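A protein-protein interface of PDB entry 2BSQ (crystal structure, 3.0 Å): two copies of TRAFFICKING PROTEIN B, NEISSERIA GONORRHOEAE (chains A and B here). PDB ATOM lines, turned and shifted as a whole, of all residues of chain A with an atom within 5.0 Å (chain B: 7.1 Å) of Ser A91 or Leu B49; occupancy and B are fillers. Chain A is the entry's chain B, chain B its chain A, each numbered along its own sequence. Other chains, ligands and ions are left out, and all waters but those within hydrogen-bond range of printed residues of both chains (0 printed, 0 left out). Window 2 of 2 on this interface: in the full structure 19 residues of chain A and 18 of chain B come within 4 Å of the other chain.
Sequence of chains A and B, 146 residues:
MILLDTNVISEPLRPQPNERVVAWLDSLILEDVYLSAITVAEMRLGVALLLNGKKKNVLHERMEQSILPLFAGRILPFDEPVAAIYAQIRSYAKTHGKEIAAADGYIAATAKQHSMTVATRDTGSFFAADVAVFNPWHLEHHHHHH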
ATOM      1  N   TYR A  86      13.982 -17.994  25.084  1.00  0.00           N
ATOM      2  CA  TYR A  86      14.551 -18.939  26.033  1.00  0.00           C
ATOM      3  C   TYR A  86      15.431 -19.941  25.279  1.00  0.00           C
ATOM      4  O   TYR A  86      16.615 -20.079  25.573  1.00  0.00           O
ATOM      5  CB  TYR A  86      13.417 -19.678  26.734  1.00  0.00           C
ATOM      6  CG  TYR A  86      13.846 -20.813  27.617  1.00  0.00           C
ATOM      7  CD1 TYR A  86      14.194 -20.587  28.929  1.00  0.00           C
ATOM      8  CD2 TYR A  86      13.892 -22.116  27.138  1.00  0.00           C
ATOM      9  CE1 TYR A  86      14.581 -21.632  29.761  1.00  0.00           C
ATOM     10  CE2 TYR A  86      14.278 -23.169  27.953  1.00  0.00           C
ATOM     11  CZ  TYR A  86      14.620 -22.918  29.270  1.00  0.00           C
ATOM     12  OH  TYR A  86      15.001 -23.933  30.121  1.00  0.00           O
ATOM     13  N   ALA A  87      14.853 -20.625  24.298  1.00  0.00           N
ATOM     14  CA  ALA A  87      15.584 -21.619  23.517  1.00  0.00           C
ATOM     15  C   ALA A  87      16.892 -21.100  22.970  1.00  0.00           C
ATOM     16  O   ALA A  87      17.910 -21.784  23.062  1.00  0.00           O
ATOM     17  CB  ALA A  87      14.729 -22.127  22.362  1.00  0.00           C
ATOM     18  N   GLN A  88      16.866 -19.908  22.376  1.00  0.00           N
ATOM     19  CA  GLN A  88      18.069 -19.306  21.813  1.00  0.00           C
ATOM     20  C   GLN A  88      19.089 -19.078  22.933  1.00  0.00           C
ATOM     21  O   GLN A  88      20.171 -19.678  22.938  1.00  0.00           O
ATOM     22  CB  GLN A  88      17.710 -17.985  21.120  1.00  0.00           C
ATOM     23  CG  GLN A  88      18.869 -17.238  20.417  1.00  0.00           C
ATOM     24  CD  GLN A  88      19.740 -16.391  21.368  1.00  0.00           C
ATOM     25  OE1 GLN A  88      19.245 -15.523  22.107  1.00  0.00           O
ATOM     26  NE2 GLN A  88      21.046 -16.636  21.331  1.00  0.00           N
ATOM     27  N   ILE A  89      18.737 -18.225  23.888  1.00  0.00           N
ATOM     28  CA  ILE A  89      19.624 -17.947  25.002  1.00  0.00           C
ATOM     29  C   ILE A  89      20.260 -19.229  25.527  1.00  0.00           C
ATOM     30  O   ILE A  89      21.472 -19.393  25.446  1.00  0.00           O
ATOM     31  CB  ILE A  89      18.879 -17.280  26.161  1.00  0.00           C
ATOM     32  CG1 ILE A  89      18.418 -15.882  25.747  1.00  0.00           C
ATOM     33  CG2 ILE A  89      19.760 -17.239  27.369  1.00  0.00           C
ATOM     34  CD1 ILE A  89      17.526 -15.194  26.753  1.00  0.00           C
ATOM     35  N   ARG A  90      19.459 -20.155  26.043  1.00  0.00           N
ATOM     36  CA  ARG A  90      20.039 -21.371  26.597  1.00  0.00           C
ATOM     37  C   ARG A  90      20.817 -22.234  25.623  1.00  0.00           C
ATOM     38  O   ARG A  90      21.935 -22.635  25.916  1.00  0.00           O
ATOM     39  CB  ARG A  90      18.983 -22.214  27.303  1.00  0.00           C
ATOM     40  CG  ARG A  90      18.616 -21.694  28.663  1.00  0.00           C
ATOM     41  CD  ARG A  90      17.897 -22.752  29.451  1.00  0.00           C
ATOM     42  NE  ARG A  90      18.816 -23.769  29.955  1.00  0.00           N
ATOM     43  CZ  ARG A  90      18.434 -24.928  30.484  1.00  0.00           C
ATOM     44  NH1 ARG A  90      17.142 -25.223  30.577  1.00  0.00           N
ATOM     45  NH2 ARG A  90      19.341 -25.796  30.924  1.00  0.00           N
ATOM     46  N   SER A  91      20.252 -22.532  24.465  1.00  0.00           N
ATOM     47  CA  SER A  91      20.985 -23.360  23.528  1.00  0.00           C
ATOM     48  C   SER A  91      22.311 -22.682  23.220  1.00  0.00           C
ATOM     49  O   SER A  91      23.352 -23.318  23.194  1.00  0.00           O
ATOM     50  CB  SER A  91      20.201 -23.545  22.241  1.00  0.00           C
ATOM     51  OG  SER A  91      20.254 -22.360  21.485  1.00  0.00           O
ATOM     52  N   TYR A  92      22.291 -21.378  23.004  1.00  0.00           N
ATOM     53  CA  TYR A  92      23.538 -20.693  22.709  1.00  0.00           C
ATOM     54  C   TYR A  92      24.622 -20.922  23.781  1.00  0.00           C
ATOM     55  O   TYR A  92      25.631 -21.575  23.532  1.00  0.00           O
ATOM     56  CB  TYR A  92      23.301 -19.197  22.550  1.00  0.00           C
ATOM     57  CG  TYR A  92      24.493 -18.516  21.953  1.00  0.00           C
ATOM     58  CD1 TYR A  92      24.668 -18.468  20.569  1.00  0.00           C
ATOM     59  CD2 TYR A  92      25.509 -18.030  22.767  1.00  0.00           C
ATOM     60  CE1 TYR A  92      25.836 -17.959  20.007  1.00  0.00           C
ATOM     61  CE2 TYR A  92      26.686 -17.522  22.222  1.00  0.00           C
ATOM     62  CZ  TYR A  92      26.849 -17.491  20.842  1.00  0.00           C
ATOM     63  OH  TYR A  92      28.035 -17.025  20.312  1.00  0.00           O
ATOM     64  N   ALA A  93      24.411 -20.369  24.972  1.00  0.00           N
ATOM     65  CA  ALA A  93      25.364 -20.509  26.070  1.00  0.00           C
ATOM     66  C   ALA A  93      25.865 -21.943  26.241  1.00  0.00           C
ATOM     67  O   ALA A  93      27.074 -22.204  26.283  1.00  0.00           O
ATOM     68  CB  ALA A  93      24.717 -20.032  27.373  1.00  0.00           C
ATOM     69  N   LYS A  94      24.917 -22.863  26.365  1.00  0.00           N
ATOM     70  CA  LYS A  94      25.228 -24.264  26.555  1.00  0.00           C
ATOM     71  C   LYS A  94      26.172 -24.781  25.494  1.00  0.00           C
ATOM     72  O   LYS A  94      27.124 -25.503  25.807  1.00  0.00           O
ATOM     73  CB  LYS A  94      23.955 -25.104  26.545  1.00  0.00           C
ATOM     74  CG  LYS A  94      23.351 -25.408  27.909  1.00  0.00           C
ATOM     75  CD  LYS A  94      22.020 -26.137  27.709  1.00  0.00           C
ATOM     76  CE  LYS A  94      21.478 -26.741  28.993  1.00  0.00           C
ATOM     77  NZ  LYS A  94      22.353 -27.836  29.521  1.00  0.00           N
ATOM     78  N   THR A  95      25.934 -24.431  24.241  1.00  0.00           N
ATOM     79  CA  THR A  95      26.836 -24.941  23.232  1.00  0.00           C
ATOM     80  C   THR A  95      28.138 -24.158  23.142  1.00  0.00           C
ATOM     81  O   THR A  95      28.925 -24.381  22.235  1.00  0.00           O
ATOM     82  CB  THR A  95      26.180 -25.031  21.829  1.00  0.00           C
ATOM     83  OG1 THR A  95      25.992 -23.722  21.286  1.00  0.00           O
ATOM     84  CG2 THR A  95      24.860 -25.755  21.907  1.00  0.00           C
ATOM     85  N   MET B  43      10.703 -27.973  23.802  1.00  0.00           N
ATOM     86  CA  MET B  43      10.808 -28.483  22.444  1.00  0.00           C
ATOM     87  C   MET B  43      11.793 -27.628  21.669  1.00  0.00           C
ATOM     88  O   MET B  43      12.750 -28.134  21.082  1.00  0.00           O
ATOM     89  CB  MET B  43       9.461 -28.411  21.740  1.00  0.00           C
ATOM     90  CG  MET B  43       8.510 -29.545  22.024  1.00  0.00           C
ATOM     91  SD  MET B  43       6.853 -29.114  21.380  1.00  0.00           S
ATOM     92  CE  MET B  43       6.991 -29.579  19.628  1.00  0.00           C
ATOM     93  N   ARG B  44      11.542 -26.326  21.666  1.00  0.00           N
ATOM     94  CA  ARG B  44      12.388 -25.386  20.950  1.00  0.00           C
ATOM     95  C   ARG B  44      13.869 -25.481  21.335  1.00  0.00           C
ATOM     96  O   ARG B  44      14.744 -25.322  20.479  1.00  0.00           O
ATOM     97  CB  ARG B  44      11.860 -23.968  21.160  1.00  0.00           C
ATOM     98  CG  ARG B  44      10.546 -23.679  20.456  1.00  0.00           C
ATOM     99  CD  ARG B  44      10.791 -22.756  19.306  1.00  0.00           C
ATOM    100  NE  ARG B  44       9.562 -22.147  18.817  1.00  0.00           N
ATOM    101  CZ  ARG B  44       8.758 -21.381  19.547  1.00  0.00           C
ATOM    102  NH1 ARG B  44       9.041 -21.120  20.814  1.00  0.00           N
ATOM    103  NH2 ARG B  44       7.671 -20.861  19.001  1.00  0.00           N
ATOM    104  N   LEU B  45      14.149 -25.746  22.609  1.00  0.00           N
ATOM    105  CA  LEU B  45      15.531 -25.880  23.077  1.00  0.00           C
ATOM    106  C   LEU B  45      16.085 -27.250  22.702  1.00  0.00           C
ATOM    107  O   LEU B  45      17.259 -27.391  22.368  1.00  0.00           O
ATOM    108  CB  LEU B  45      15.619 -25.712  24.601  1.00  0.00           C
ATOM    109  CG  LEU B  45      16.956 -26.074  25.263  1.00  0.00           C
ATOM    110  CD1 LEU B  45      18.054 -25.282  24.621  1.00  0.00           C
ATOM    111  CD2 LEU B  45      16.913 -25.789  26.747  1.00  0.00           C
ATOM    112  N   GLY B  46      15.236 -28.264  22.768  1.00  0.00           N
ATOM    113  CA  GLY B  46      15.684 -29.600  22.431  1.00  0.00           C
ATOM    114  C   GLY B  46      16.172 -29.680  21.001  1.00  0.00           C
ATOM    115  O   GLY B  46      17.018 -30.510  20.660  1.00  0.00           O
ATOM    116  N   VAL B  47      15.614 -28.823  20.154  1.00  0.00           N
ATOM    117  CA  VAL B  47      15.999 -28.791  18.757  1.00  0.00           C
ATOM    118  C   VAL B  47      17.312 -28.027  18.668  1.00  0.00           C
ATOM    119  O   VAL B  47      18.306 -28.538  18.151  1.00  0.00           O
ATOM    120  CB  VAL B  47      14.914 -28.094  17.906  1.00  0.00           C
ATOM    121  CG1 VAL B  47      15.421 -27.845  16.491  1.00  0.00           C
ATOM    122  CG2 VAL B  47      13.675 -28.957  17.865  1.00  0.00           C
ATOM    123  N   ALA B  48      17.312 -26.812  19.202  1.00  0.00           N
ATOM    124  CA  ALA B  48      18.494 -25.962  19.198  1.00  0.00           C
ATOM    125  C   ALA B  48      19.788 -26.659  19.642  1.00  0.00           C
ATOM    126  O   ALA B  48      20.874 -26.320  19.164  1.00  0.00           O
ATOM    127  CB  ALA B  48      18.239 -24.764  20.077  1.00  0.00           C
ATOM    128  N   LEU B  49      19.674 -27.628  20.547  1.00  0.00           N
ATOM    129  CA  LEU B  49      20.846 -28.327  21.062  1.00  0.00           C
ATOM    130  C   LEU B  49      21.461 -29.406  20.176  1.00  0.00           C
ATOM    131  O   LEU B  49      22.498 -29.962  20.527  1.00  0.00           O
ATOM    132  CB  LEU B  49      20.541 -28.939  22.430  1.00  0.00           C
ATOM    133  CG  LEU B  49      20.351 -28.008  23.626  1.00  0.00           C
ATOM    134  CD1 LEU B  49      19.996 -28.825  24.844  1.00  0.00           C
ATOM    135  CD2 LEU B  49      21.613 -27.223  23.890  1.00  0.00           C
ATOM    136  N   LEU B  50      20.842 -29.711  19.043  1.00  0.00           N
ATOM    137  CA  LEU B  50      21.373 -30.736  18.142  1.00  0.00           C
ATOM    138  C   LEU B  50      22.588 -30.218  17.374  1.00  0.00           C
ATOM    139  O   LEU B  50      22.664 -29.016  17.087  1.00  0.00           O
ATOM    140  CB  LEU B  50      20.303 -31.153  17.127  1.00  0.00           C
ATOM    141  CG  LEU B  50      19.151 -32.053  17.573  1.00  0.00           C
ATOM    142  CD1 LEU B  50      18.169 -32.206  16.431  1.00  0.00           C
ATOM    143  CD2 LEU B  50      19.689 -33.411  18.011  1.00  0.00           C
ATOM    144  N   LEU B  51      23.529 -31.107  17.034  1.00  0.00           N
ATOM    145  CA  LEU B  51      24.711 -30.702  16.264  1.00  0.00           C
ATOM    146  C   LEU B  51      24.255 -30.157  14.911  1.00  0.00           C
ATOM    147  O   LEU B  51      23.363 -30.712  14.262  1.00  0.00           O
ATOM    148  CB  LEU B  51      25.660 -31.881  16.018  1.00  0.00           C
ATOM    149  CG  LEU B  51      26.319 -32.607  17.194  1.00  0.00           C
ATOM    150  CD1 LEU B  51      27.448 -33.490  16.687  1.00  0.00           C
ATOM    151  CD2 LEU B  51      26.861 -31.598  18.183  1.00  0.00           C
ATOM    152  N   ASN B  52      24.878 -29.072  14.480  1.00  0.00           N
ATOM    153  CA  ASN B  52      24.519 -28.454  13.215  1.00  0.00           C
ATOM    154  C   ASN B  52      24.664 -29.388  12.027  1.00  0.00           C
ATOM    155  O   ASN B  52      25.738 -29.917  11.755  1.00  0.00           O
ATOM    156  CB  ASN B  52      25.347 -27.188  13.018  1.00  0.00           C
ATOM    157  CG  ASN B  52      24.871 -26.052  13.904  1.00  0.00           C
ATOM    158  OD1 ASN B  52      23.942 -25.324  13.546  1.00  0.00           O
ATOM    159  ND2 ASN B  52      25.484 -25.909  15.079  1.00  0.00           N
ATOM    160  N   LYS B  56      18.854 -31.195  11.802  1.00  0.00           N
ATOM    161  CA  LYS B  56      18.429 -30.108  12.668  1.00  0.00           C
ATOM    162  C   LYS B  56      17.744 -28.965  11.935  1.00  0.00           C
ATOM    163  O   LYS B  56      16.875 -28.309  12.497  1.00  0.00           O
ATOM    164  CB  LYS B  56      19.619 -29.577  13.463  1.00  0.00           C
ATOM    165  CG  LYS B  56      19.342 -28.290  14.182  1.00  0.00           C
ATOM    166  CD  LYS B  56      20.524 -27.892  15.021  1.00  0.00           C
ATOM    167  CE  LYS B  56      20.403 -26.453  15.466  1.00  0.00           C
ATOM    168  NZ  LYS B  56      21.508 -26.083  16.386  1.00  0.00           N
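The backbone carbonyl oxygen (O) of Ala B48 sits at hydrogen-bond distance from the side-chain amino group (NZ) of Lys B56 (2.9 Å). O of Gln A88 sits at hydrogen-bond distance from OG of Ser A91 (3.1 Å). O of Ala A87 sits at hydrogen-bond distance from OG of Ser A91, 2.9 Å away. The side-chain hydroxyl of Tyr A86 sits at hydrogen-bond distance from the guanidinium group of Arg A90 (2.5 Å). The backbone carbonyl oxygen (O) of Ser A91 sits close to the side-chain hydroxyl (OG1) of Thr A95 (3.3 Å).
Among the printed residues, pairs that only touch across the chains: Tyr A86 with Leu B45, Ala A87 with Arg B44, Ala A87 with Leu B45, Arg A90 with Leu B45, Ser A91 with Leu B45, Ser A91 with Ala B48, Ser A91 with Leu B49 and Lys A94 with Leu B49.
Of chain B, only Leu B45, Ala B48 and Leu B49 come within 4 Å of Ser A91. Printed residues of chain A within 4 Å of Leu B49: Ser A91 and Lys A94. Printed residues of chain A within 4 Å of Leu B45: Tyr A86, Ala A87, Arg A90 and Ser A91. Printed residues of chain B within 4 Å of Ala A87: Arg B44 (3.6 Å) and Leu B45 (3.7 Å). Printed residues of chain B within 4 Å of Lys A94: Leu B49 (3.99 Å). Of the printed residues of chain A, Ala B48 touches Ser A91 (3.2 Å). Gly B46 touches none of the printed residues of chain A. Thr A95 touches none of the printed residues of chain B. The nearest printed residue of chain A that does not touch Arg B44 is Ser A91 (6.0 Å).
Of the 10 printed residues of chain A, 5 touch a printed residue of chain B. Printed residues of chain A that touch a printed residue of chain B: Tyr A86, Ala A87, Arg A90, Ser A91 and Lys A94. Hydrophobic or aromatic side chains of chain A that line the printed part of chain B: Tyr A86 and Ala A87. Of the 11 printed residues of chain B, 4 touch a printed residue of chain A. Hydrophobic or aromatic side chains of chain B within 4 Å of the printed part of chain A: Leu B45, Ala B48 and Leu B49.
No position is printed for both chains. Of the 8 pairs that touch across the chains among the printed residues, none has its exchanged pair printed and touching as well.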
